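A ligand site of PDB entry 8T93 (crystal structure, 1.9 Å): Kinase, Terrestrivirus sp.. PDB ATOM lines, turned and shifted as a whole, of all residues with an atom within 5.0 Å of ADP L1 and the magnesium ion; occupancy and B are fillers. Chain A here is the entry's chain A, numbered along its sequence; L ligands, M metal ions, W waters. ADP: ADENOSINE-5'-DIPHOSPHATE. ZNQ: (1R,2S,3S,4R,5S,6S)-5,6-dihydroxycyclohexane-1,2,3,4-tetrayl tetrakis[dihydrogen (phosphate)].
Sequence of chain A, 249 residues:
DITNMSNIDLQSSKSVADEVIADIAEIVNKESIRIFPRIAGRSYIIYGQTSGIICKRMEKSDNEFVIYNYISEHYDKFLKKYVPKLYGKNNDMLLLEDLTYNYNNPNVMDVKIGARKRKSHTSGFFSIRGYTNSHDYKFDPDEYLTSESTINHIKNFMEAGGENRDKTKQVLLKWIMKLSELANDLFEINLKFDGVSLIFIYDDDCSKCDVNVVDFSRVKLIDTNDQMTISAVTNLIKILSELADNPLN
The side-chain carboxylate (OD2) of Asp 110 sits at hydrogen-bond distance from an oxygen (O3') of ADP L1 (2.6 Å).
O of Glu 97 is in hydrogen-bond range of N6 of ADP L1, 2.7 Å away.
O2B of ADP L1 sits at hydrogen-bond distance from N of Ser 43, at 2.9 Å.
The side-chain hydroxyl (OG) of Ser 43 is in hydrogen-bond range of an oxygen (O3B) of ADP L1, at 3.2 Å.
An oxygen (O2') of ADP L1 is in hydrogen-bond range of the backbone NH (N) of Ile 39.
O2A of ADP L1 lies within salt-bridge range of NZ of Lys 56 (2.9 Å).
N of Leu 99 is in hydrogen-bond range of N1 of ADP L1.
The backbone NH (N) of Arg 42 lies within hydrogen-bond range of an oxygen (O2B) of ADP L1 (3.1 Å).
O3' of ADP L1 is in hydrogen-bond range of N of Ala 40 (3.2 Å).
O13 of ZNQ L2 lies within hydrogen-bond range of NH1 of Arg 42, 3.1 Å away.
The magnesium ion is bound by O1A of ADP L1 (2.0 Å), water W3 (2.0 Å), O1B of ADP L1 (2.1 Å), water W1 (2.1 Å), OD2 of Asp 215 (2.1 Å) and water W4 (2.1 Å).
Water W4 lies within hydrogen-bond range of OG of Ser 197 and O of Gly 195.
Merely in contact with ADP L1: Gly 41, Ile 54, Phe 36, Ile 45, Pro 84, Asp 98, Val 214, Arg 38 and Ile 199.
Hydrophobic or aromatic side chains that line ADP L1: Phe 36, Ile 39, Ala 40, Ile 45, Ile 54, Pro 84, Leu 99, Ile 199 and Val 214.
Within 4 Å of ADP L1: Phe 36, Arg 38, Ile 39, Ala 40, Gly 41, Arg 42, Ser 43, Ile 45, Ile 54, Lys 56, Pro 84, Glu 97, Asp 98, Leu 99, Asp 110, Ile 199, Val 214 and Asp 215.
The nearest printed residue that does not touch ADP L1 is Leu 96 (4.2 Å).
The side-chain amino group (NZ) of Lys 56 lies within salt-bridge range of the side-chain carboxylate (OD1) of Asp 215 (3.5 Å).
The side-chain carboxylate of Asp 215 is in hydrogen-bond range of the side-chain hydroxyl of Ser 217 (2.6 Å).
The side-chain carboxylate (OD1) of Asp 110 sits at hydrogen-bond distance from the side-chain hydroxyl (OG) of Ser 197, 2.5 Å away.
O of Ser 43 is in hydrogen-bond range of NE of Arg 38 (3.2 Å).
NZ of Lys 56 is in salt-bridge range of OE1 of Glu 64 (2.9 Å).
N of Phe 36 is in hydrogen-bond range of O of Ile 45 (3.1 Å).
OG1 of Thr 100 sits at hydrogen-bond distance from OD1 of Asp 98 (2.6 Å).
The backbone carbonyl oxygen (O) of Ser 197 sits at hydrogen-bond distance from the backbone NH (N) of Val 214 (2.9 Å).
Of the 26 residues printed, 1 comes within 4 Å of the magnesium ion.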
ATOM      1  N   PHE A  36       3.507  -6.677   8.118  1.00  0.00           N
ATOM      2  CA  PHE A  36       3.089  -7.190   6.791  1.00  0.00           C
ATOM      3  C   PHE A  36       4.304  -7.758   6.052  1.00  0.00           C
ATOM      4  O   PHE A  36       5.344  -7.109   6.019  1.00  0.00           O
ATOM      5  CB  PHE A  36       2.445  -6.051   6.006  1.00  0.00           C
ATOM      6  CG  PHE A  36       1.792  -6.570   4.754  1.00  0.00           C
ATOM      7  CD1 PHE A  36       0.623  -7.323   4.830  1.00  0.00           C
ATOM      8  CD2 PHE A  36       2.360  -6.353   3.513  1.00  0.00           C
ATOM      9  CE1 PHE A  36       0.015  -7.827   3.683  1.00  0.00           C
ATOM     10  CE2 PHE A  36       1.747  -6.836   2.370  1.00  0.00           C
ATOM     11  CZ  PHE A  36       0.585  -7.580   2.456  1.00  0.00           C
ATOM     12  N   PRO A  37       4.256  -8.932   5.399  1.00  0.00           N
ATOM     13  CA  PRO A  37       5.402  -9.408   4.601  1.00  0.00           C
ATOM     14  C   PRO A  37       5.620  -8.626   3.287  1.00  0.00           C
ATOM     15  O   PRO A  37       5.172  -9.030   2.235  1.00  0.00           O
ATOM     16  CB  PRO A  37       5.016 -10.877   4.321  1.00  0.00           C
ATOM     17  CG  PRO A  37       3.472 -10.837   4.238  1.00  0.00           C
ATOM     18  CD  PRO A  37       3.084  -9.843   5.336  1.00  0.00           C
ATOM     19  N   ARG A  38       6.329  -7.507   3.367  1.00  0.00           N
ATOM     20  CA  ARG A  38       6.657  -6.575   2.239  1.00  0.00           C
ATOM     21  C   ARG A  38       7.564  -7.343   1.261  1.00  0.00           C
ATOM     22  O   ARG A  38       8.419  -8.107   1.721  1.00  0.00           O
ATOM     23  CB  ARG A  38       7.418  -5.334   2.735  1.00  0.00           C
ATOM     24  CG  ARG A  38       6.547  -4.358   3.492  1.00  0.00           C
ATOM     25  CD  ARG A  38       7.228  -3.179   4.182  1.00  0.00           C
ATOM     26  NE  ARG A  38       8.548  -2.847   3.711  1.00  0.00           N
ATOM     27  CZ  ARG A  38       9.645  -2.921   4.459  1.00  0.00           C
ATOM     28  NH1 ARG A  38       9.594  -3.320   5.722  1.00  0.00           N
ATOM     29  NH2 ARG A  38      10.812  -2.570   3.951  1.00  0.00           N
ATOM     30  N   ILE A  39       7.451  -7.097  -0.049  1.00  0.00           N
ATOM     31  CA  ILE A  39       8.401  -7.649  -1.044  1.00  0.00           C
ATOM     32  C   ILE A  39       9.587  -6.683  -1.118  1.00  0.00           C
ATOM     33  O   ILE A  39      10.708  -7.176  -1.223  1.00  0.00           O
ATOM     34  CB  ILE A  39       7.692  -7.901  -2.399  1.00  0.00           C
ATOM     35  CG1 ILE A  39       6.883  -9.197  -2.348  1.00  0.00           C
ATOM     36  CG2 ILE A  39       8.699  -7.975  -3.531  1.00  0.00           C
ATOM     37  CD1 ILE A  39       7.705 -10.405  -1.906  1.00  0.00           C
ATOM     38  N   ALA A  40       9.373  -5.369  -1.146  1.00  0.00           N
ATOM     39  CA  ALA A  40      10.439  -4.357  -1.352  1.00  0.00           C
ATOM     40  C   ALA A  40      10.145  -3.062  -0.579  1.00  0.00           C
ATOM     41  O   ALA A  40       9.128  -3.028   0.165  1.00  0.00           O
ATOM     42  CB  ALA A  40      10.601  -4.099  -2.836  1.00  0.00           C
ATOM     43  N   GLY A  41      10.976  -2.043  -0.772  1.00  0.00           N
ATOM     44  CA  GLY A  41      10.803  -0.697  -0.166  1.00  0.00           C
ATOM     45  C   GLY A  41      11.198  -0.723   1.308  1.00  0.00           C
ATOM     46  O   GLY A  41      11.672  -1.730   1.756  1.00  0.00           O
ATOM     47  N   ARG A  42      10.976   0.360   2.057  1.00  0.00           N
ATOM     48  CA  ARG A  42      11.558   0.582   3.411  1.00  0.00           C
ATOM     49  C   ARG A  42      10.492   1.048   4.415  1.00  0.00           C
ATOM     50  O   ARG A  42      10.797   1.119   5.635  1.00  0.00           O
ATOM     51  CB  ARG A  42      12.639   1.675   3.361  1.00  0.00           C
ATOM     52  CG  ARG A  42      13.817   1.361   2.466  1.00  0.00           C
ATOM     53  CD  ARG A  42      15.045   2.213   2.812  1.00  0.00           C
ATOM     54  NE  ARG A  42      16.124   1.863   1.884  1.00  0.00           N
ATOM     55  CZ  ARG A  42      17.220   2.590   1.670  1.00  0.00           C
ATOM     56  NH1 ARG A  42      17.412   3.728   2.318  1.00  0.00           N
ATOM     57  NH2 ARG A  42      18.129   2.177   0.794  1.00  0.00           N
ATOM     58  N   SER A  43       9.278   1.365   3.949  1.00  0.00           N
ATOM     59  CA  SER A  43       8.227   1.948   4.814  1.00  0.00           C
ATOM     60  C   SER A  43       7.752   0.885   5.785  1.00  0.00           C
ATOM     61  O   SER A  43       7.777  -0.282   5.450  1.00  0.00           O
ATOM     62  CB  SER A  43       7.080   2.553   4.019  1.00  0.00           C
ATOM     63  OG  SER A  43       7.535   3.711   3.327  1.00  0.00           O
ATOM     64  N   ILE A  45       4.984  -1.042   7.281  1.00  0.00           N
ATOM     65  CA  ILE A  45       3.650  -1.543   6.852  1.00  0.00           C
ATOM     66  C   ILE A  45       3.302  -2.687   7.775  1.00  0.00           C
ATOM     67  O   ILE A  45       4.111  -3.618   7.885  1.00  0.00           O
ATOM     68  CB  ILE A  45       3.613  -1.968   5.377  1.00  0.00           C
ATOM     69  CG1 ILE A  45       4.088  -0.797   4.507  1.00  0.00           C
ATOM     70  CG2 ILE A  45       2.224  -2.502   5.049  1.00  0.00           C
ATOM     71  CD1 ILE A  45       4.323  -1.104   3.014  1.00  0.00           C
ATOM     72  N   ILE A  54      -4.223  -3.033   5.072  1.00  0.00           N
ATOM     73  CA  ILE A  54      -2.840  -2.837   5.581  1.00  0.00           C
ATOM     74  C   ILE A  54      -2.698  -1.383   5.947  1.00  0.00           C
ATOM     75  O   ILE A  54      -3.442  -0.570   5.378  1.00  0.00           O
ATOM     76  CB  ILE A  54      -1.790  -3.298   4.561  1.00  0.00           C
ATOM     77  CG1 ILE A  54      -1.920  -2.562   3.230  1.00  0.00           C
ATOM     78  CG2 ILE A  54      -1.882  -4.806   4.405  1.00  0.00           C
ATOM     79  CD1 ILE A  54      -0.646  -2.663   2.340  1.00  0.00           C
ATOM     80  N   LYS A  56       0.033   1.628   6.131  1.00  0.00           N
ATOM     81  CA  LYS A  56       1.355   2.055   5.609  1.00  0.00           C
ATOM     82  C   LYS A  56       1.677   3.377   6.256  1.00  0.00           C
ATOM     83  O   LYS A  56       0.897   4.347   6.056  1.00  0.00           O
ATOM     84  CB  LYS A  56       1.396   2.138   4.091  1.00  0.00           C
ATOM     85  CG  LYS A  56       2.632   2.815   3.539  1.00  0.00           C
ATOM     86  CD  LYS A  56       2.702   2.870   2.028  1.00  0.00           C
ATOM     87  CE  LYS A  56       3.993   3.526   1.625  1.00  0.00           C
ATOM     88  NZ  LYS A  56       4.092   3.623   0.162  1.00  0.00           N
ATOM     89  N   GLU A  64       2.214  11.259  -0.087  1.00  0.00           N
ATOM     90  CA  GLU A  64       1.467  10.101  -0.652  1.00  0.00           C
ATOM     91  C   GLU A  64      -0.055  10.351  -0.499  1.00  0.00           C
ATOM     92  O   GLU A  64      -0.813  10.124  -1.467  1.00  0.00           O
ATOM     93  CB  GLU A  64       1.886   8.788  -0.001  1.00  0.00           C
ATOM     94  CG  GLU A  64       1.311   7.616  -0.760  1.00  0.00           C
ATOM     95  CD  GLU A  64       1.971   6.265  -0.558  1.00  0.00           C
ATOM     96  OE1 GLU A  64       2.766   6.143   0.401  1.00  0.00           O
ATOM     97  OE2 GLU A  64       1.719   5.337  -1.423  1.00  0.00           O
ATOM     98  N   PRO A  84      -4.750   0.370  -5.366  1.00  0.00           N
ATOM     99  CA  PRO A  84      -5.463  -0.128  -4.186  1.00  0.00           C
ATOM    100  C   PRO A  84      -6.332   1.013  -3.632  1.00  0.00           C
ATOM    101  O   PRO A  84      -5.929   2.183  -3.659  1.00  0.00           O
ATOM    102  CB  PRO A  84      -4.364  -0.544  -3.208  1.00  0.00           C
ATOM    103  CG  PRO A  84      -3.134   0.222  -3.659  1.00  0.00           C
ATOM    104  CD  PRO A  84      -3.292   0.304  -5.179  1.00  0.00           C
ATOM    105  N   LEU A  96      -5.040   0.960   3.579  1.00  0.00           N
ATOM    106  CA  LEU A  96      -5.072   0.573   2.151  1.00  0.00           C
ATOM    107  C   LEU A  96      -5.642  -0.816   2.025  1.00  0.00           C
ATOM    108  O   LEU A  96      -5.413  -1.682   2.937  1.00  0.00           O
ATOM    109  CB  LEU A  96      -3.661   0.566   1.578  1.00  0.00           C
ATOM    110  CG  LEU A  96      -2.990   1.929   1.502  1.00  0.00           C
ATOM    111  CD1 LEU A  96      -1.536   1.763   1.020  1.00  0.00           C
ATOM    112  CD2 LEU A  96      -3.733   2.792   0.520  1.00  0.00           C
ATOM    113  N   GLU A  97      -6.313  -1.028   0.909  1.00  0.00           N
ATOM    114  CA  GLU A  97      -6.692  -2.365   0.431  1.00  0.00           C
ATOM    115  C   GLU A  97      -5.449  -3.254   0.420  1.00  0.00           C
ATOM    116  O   GLU A  97      -4.460  -2.902  -0.259  1.00  0.00           O
ATOM    117  CB  GLU A  97      -7.323  -2.243  -0.943  1.00  0.00           C
ATOM    118  CG  GLU A  97      -7.768  -3.558  -1.544  1.00  0.00           C
ATOM    119  CD  GLU A  97      -8.171  -3.407  -2.998  1.00  0.00           C
ATOM    120  OE1 GLU A  97      -8.168  -2.266  -3.569  1.00  0.00           O
ATOM    121  OE2 GLU A  97      -8.402  -4.466  -3.598  1.00  0.00           O
ATOM    122  N   ASP A  98      -5.551  -4.406   1.080  1.00  0.00           N
ATOM    123  CA  ASP A  98      -4.532  -5.473   0.997  1.00  0.00           C
ATOM    124  C   ASP A  98      -4.762  -6.218  -0.334  1.00  0.00           C
ATOM    125  O   ASP A  98      -5.682  -7.034  -0.455  1.00  0.00           O
ATOM    126  CB  ASP A  98      -4.619  -6.386   2.190  1.00  0.00           C
ATOM    127  CG  ASP A  98      -3.654  -7.544   2.135  1.00  0.00           C
ATOM    128  OD1 ASP A  98      -2.880  -7.639   1.150  1.00  0.00           O
ATOM    129  OD2 ASP A  98      -3.637  -8.308   3.118  1.00  0.00           O
ATOM    130  N   LEU A  99      -3.862  -5.995  -1.299  1.00  0.00           N
ATOM    131  CA  LEU A  99      -3.966  -6.595  -2.645  1.00  0.00           C
ATOM    132  C   LEU A  99      -3.733  -8.111  -2.589  1.00  0.00           C
ATOM    133  O   LEU A  99      -4.032  -8.783  -3.583  1.00  0.00           O
ATOM    134  CB  LEU A  99      -2.934  -5.911  -3.572  1.00  0.00           C
ATOM    135  CG  LEU A  99      -3.170  -4.424  -3.868  1.00  0.00           C
ATOM    136  CD1 LEU A  99      -1.959  -3.854  -4.641  1.00  0.00           C
ATOM    137  CD2 LEU A  99      -4.434  -4.221  -4.697  1.00  0.00           C
ATOM    138  N   THR A 100      -3.206  -8.648  -1.482  1.00  0.00           N
ATOM    139  CA  THR A 100      -2.947 -10.112  -1.363  1.00  0.00           C
ATOM    140  C   THR A 100      -4.107 -10.815  -0.661  1.00  0.00           C
ATOM    141  O   THR A 100      -4.084 -12.062  -0.597  1.00  0.00           O
ATOM    142  CB  THR A 100      -1.677 -10.408  -0.549  1.00  0.00           C
ATOM    143  OG1 THR A 100      -1.791 -10.001   0.806  1.00  0.00           O
ATOM    144  CG2 THR A 100      -0.461  -9.725  -1.125  1.00  0.00           C
ATOM    145  N   VAL A 108       4.003 -12.506  -5.216  1.00  0.00           N
ATOM    146  CA  VAL A 108       4.039 -11.038  -5.453  1.00  0.00           C
ATOM    147  C   VAL A 108       5.372 -10.631  -6.046  1.00  0.00           C
ATOM    148  O   VAL A 108       6.393 -11.137  -5.567  1.00  0.00           O
ATOM    149  CB  VAL A 108       3.817 -10.271  -4.136  1.00  0.00           C
ATOM    150  CG1 VAL A 108       3.745  -8.776  -4.383  1.00  0.00           C
ATOM    151  CG2 VAL A 108       2.592 -10.793  -3.426  1.00  0.00           C
ATOM    152  N   ASP A 110       7.325  -6.901  -7.098  1.00  0.00           N
ATOM    153  CA  ASP A 110       7.370  -5.438  -7.060  1.00  0.00           C
ATOM    154  C   ASP A 110       8.304  -5.019  -8.192  1.00  0.00           C
ATOM    155  O   ASP A 110       9.508  -5.376  -8.115  1.00  0.00           O
ATOM    156  CB  ASP A 110       7.834  -4.928  -5.698  1.00  0.00           C
ATOM    157  CG  ASP A 110       7.894  -3.403  -5.549  1.00  0.00           C
ATOM    158  OD1 ASP A 110       8.195  -2.698  -6.527  1.00  0.00           O
ATOM    159  OD2 ASP A 110       7.648  -2.931  -4.425  1.00  0.00           O
ATOM    160  N   GLY A 195       9.191   6.917  -8.616  1.00  0.00           N
ATOM    161  CA  GLY A 195       9.269   5.916  -7.539  1.00  0.00           C
ATOM    162  C   GLY A 195       8.081   4.955  -7.528  1.00  0.00           C
ATOM    163  O   GLY A 195       8.067   4.069  -6.637  1.00  0.00           O
ATOM    164  N   SER A 197       5.612   1.779  -8.228  1.00  0.00           N
ATOM    165  CA  SER A 197       5.822   0.347  -8.527  1.00  0.00           C
ATOM    166  C   SER A 197       4.529  -0.315  -9.038  1.00  0.00           C
ATOM    167  O   SER A 197       3.467   0.152  -8.712  1.00  0.00           O
ATOM    168  CB  SER A 197       6.273  -0.404  -7.294  1.00  0.00           C
ATOM    169  OG  SER A 197       7.638  -0.304  -7.050  1.00  0.00           O
ATOM    170  N   ILE A 199       2.611  -3.838  -8.625  1.00  0.00           N
ATOM    171  CA  ILE A 199       2.579  -5.038  -7.760  1.00  0.00           C
ATOM    172  C   ILE A 199       1.848  -6.127  -8.547  1.00  0.00           C
ATOM    173  O   ILE A 199       0.657  -6.018  -8.697  1.00  0.00           O
ATOM    174  CB  ILE A 199       1.918  -4.721  -6.399  1.00  0.00           C
ATOM    175  CG1 ILE A 199       2.665  -3.613  -5.669  1.00  0.00           C
ATOM    176  CG2 ILE A 199       1.799  -5.990  -5.577  1.00  0.00           C
ATOM    177  CD1 ILE A 199       4.121  -3.837  -5.590  1.00  0.00           C
ATOM    178  N   VAL A 214       1.293   1.176  -7.083  1.00  0.00           N
ATOM    179  CA  VAL A 214       1.400   1.586  -5.646  1.00  0.00           C
ATOM    180  C   VAL A 214       2.578   2.561  -5.469  1.00  0.00           C
ATOM    181  O   VAL A 214       3.450   2.633  -6.359  1.00  0.00           O
ATOM    182  CB  VAL A 214       1.525   0.374  -4.713  1.00  0.00           C
ATOM    183  CG1 VAL A 214       0.420  -0.648  -4.956  1.00  0.00           C
ATOM    184  CG2 VAL A 214       2.939  -0.235  -4.791  1.00  0.00           C
ATOM    185  N   ASP A 215       2.551   3.257  -4.341  1.00  0.00           N
ATOM    186  CA  ASP A 215       3.658   4.057  -3.797  1.00  0.00           C
ATOM    187  C   ASP A 215       3.696   5.402  -4.481  1.00  0.00           C
ATOM    188  O   ASP A 215       4.518   5.591  -5.401  1.00  0.00           O
ATOM    189  CB  ASP A 215       5.027   3.402  -3.961  1.00  0.00           C
ATOM    190  CG  ASP A 215       6.067   4.068  -3.067  1.00  0.00           C
ATOM    191  OD1 ASP A 215       5.709   5.152  -2.494  1.00  0.00           O
ATOM    192  OD2 ASP A 215       7.205   3.477  -2.934  1.00  0.00           O
ATOM    193  N   SER A 217       4.517   8.176  -2.932  1.00  0.00           N
ATOM    194  CA  SER A 217       5.293   9.030  -1.980  1.00  0.00           C
ATOM    195  C   SER A 217       6.126  10.095  -2.716  1.00  0.00           C
ATOM    196  O   SER A 217       6.191  11.219  -2.185  1.00  0.00           O
ATOM    197  CB  SER A 217       6.131   8.217  -1.037  1.00  0.00           C
ATOM    198  OG  SER A 217       6.973   7.337  -1.727  1.00  0.00           O
HETATM  199  PB  ADP L   1       7.666   1.823   0.060  1.00  0.00           P
HETATM  200  O1B ADP L   1       8.533   1.551  -1.167  1.00  0.00           O
HETATM  201  O2B ADP L   1       8.094   1.191   1.308  1.00  0.00           O
HETATM  202  O3B ADP L   1       7.325   3.400   0.170  1.00  0.00           O
HETATM  203  PA  ADP L   1       5.406   0.593  -1.411  1.00  0.00           P
HETATM  204  O1A ADP L   1       6.303   0.632  -2.605  1.00  0.00           O
HETATM  205  O2A ADP L   1       4.026   1.211  -1.473  1.00  0.00           O
HETATM  206  O3A ADP L   1       6.146   1.181  -0.117  1.00  0.00           O
HETATM  207  O5' ADP L   1       5.205  -0.927  -0.949  1.00  0.00           O
HETATM  208  C5' ADP L   1       6.286  -1.740  -0.417  1.00  0.00           C
HETATM  209  C4' ADP L   1       5.824  -3.170  -0.470  1.00  0.00           C
HETATM  210  O4' ADP L   1       4.568  -3.302   0.241  1.00  0.00           O
HETATM  211  C3' ADP L   1       5.502  -3.702  -1.877  1.00  0.00           C
HETATM  212  O3' ADP L   1       6.662  -4.284  -2.470  1.00  0.00           O
HETATM  213  C2' ADP L   1       4.433  -4.769  -1.591  1.00  0.00           C
HETATM  214  O2' ADP L   1       5.030  -5.990  -1.208  1.00  0.00           O
HETATM  215  C1' ADP L   1       3.687  -4.196  -0.399  1.00  0.00           C
HETATM  216  N9  ADP L   1       2.460  -3.450  -0.704  1.00  0.00           N
HETATM  217  C8  ADP L   1       2.277  -2.088  -0.822  1.00  0.00           C
HETATM  218  N7  ADP L   1       1.019  -1.732  -1.009  1.00  0.00           N
HETATM  219  C5  ADP L   1       0.335  -2.927  -0.925  1.00  0.00           C
HETATM  220  C6  ADP L   1      -1.023  -3.202  -0.993  1.00  0.00           C
HETATM  221  N6  ADP L   1      -1.958  -2.229  -1.114  1.00  0.00           N
HETATM  222  N1  ADP L   1      -1.372  -4.495  -0.842  1.00  0.00           N
HETATM  223  C2  ADP L   1      -0.428  -5.432  -0.664  1.00  0.00           C
HETATM  224  N3  ADP L   1       0.902  -5.303  -0.608  1.00  0.00           N
HETATM  225  C4  ADP L   1       1.215  -4.003  -0.744  1.00  0.00           C
HETATM  226  O21 ZNQ L   2      13.105   1.925  -0.803  1.00  0.00           O
HETATM  227  P1  ZNQ L   2      13.543   1.911  -2.373  1.00  0.00           P
HETATM  228  O41 ZNQ L   2      14.400   0.719  -2.651  1.00  0.00           O
HETATM  229  O31 ZNQ L   2      12.126   1.772  -3.248  1.00  0.00           O
HETATM  230  O11 ZNQ L   2      14.212   3.389  -2.906  1.00  0.00           O
HETATM  231  C1  ZNQ L   2      15.340   3.852  -2.309  1.00  0.00           C
HETATM  232  C6  ZNQ L   2      16.041   4.562  -3.337  1.00  0.00           C
HETATM  233  O16 ZNQ L   2      16.286   3.579  -4.360  1.00  0.00           O
HETATM  234  P6  ZNQ L   2      15.991   4.016  -5.877  1.00  0.00           P
HETATM  235  O46 ZNQ L   2      15.049   5.353  -6.031  1.00  0.00           O
HETATM  236  O26 ZNQ L   2      17.358   4.045  -6.525  1.00  0.00           O
HETATM  237  O36 ZNQ L   2      15.001   2.727  -6.533  1.00  0.00           O
HETATM  238  C5  ZNQ L   2      17.427   5.041  -2.929  1.00  0.00           C
HETATM  239  O15 ZNQ L   2      17.781   5.870  -3.985  1.00  0.00           O
HETATM  240  P5  ZNQ L   2      19.202   5.951  -4.721  1.00  0.00           P
HETATM  241  O45 ZNQ L   2      18.905   6.278  -6.317  1.00  0.00           O
HETATM  242  O35 ZNQ L   2      19.723   7.325  -4.021  1.00  0.00           O
HETATM  243  O25 ZNQ L   2      19.956   4.720  -4.299  1.00  0.00           O
HETATM  244  C2  ZNQ L   2      15.011   4.732  -1.077  1.00  0.00           C
HETATM  245  O12 ZNQ L   2      14.482   3.929   0.133  1.00  0.00           O
HETATM  246  C3  ZNQ L   2      16.466   5.211  -0.608  1.00  0.00           C
HETATM  247  O13 ZNQ L   2      16.276   5.999   0.528  1.00  0.00           O
HETATM  248  C4  ZNQ L   2      17.267   5.938  -1.671  1.00  0.00           C
HETATM  249  O14 ZNQ L   2      18.637   6.325  -1.195  1.00  0.00           O
HETATM  250  P4  ZNQ L   2      18.893   7.752  -0.444  1.00  0.00           P
HETATM  251  O24 ZNQ L   2      18.037   8.785  -1.145  1.00  0.00           O
HETATM  252  O44 ZNQ L   2      20.537   7.996  -0.357  1.00  0.00           O
HETATM  253  O34 ZNQ L   2      18.484   7.458   1.158  1.00  0.00           O
HETATM  254 MG    MG M   1       8.011   1.541  -3.157  1.00  0.00          MG
HETATM  255  O   HOH W   1       8.790  -0.380  -3.541  1.00  0.00           O
HETATM  256  O   HOH W   2       1.394   1.068  -1.086  1.00  0.00           O
HETATM  257  O   HOH W   3       9.843   2.378  -3.497  1.00  0.00           O
HETATM  258  O   HOH W   4       7.691   1.681  -5.255  1.00  0.00           O
HETATM  259  O   HOH W   5       2.777  -7.519  -1.026  1.00  0.00           O
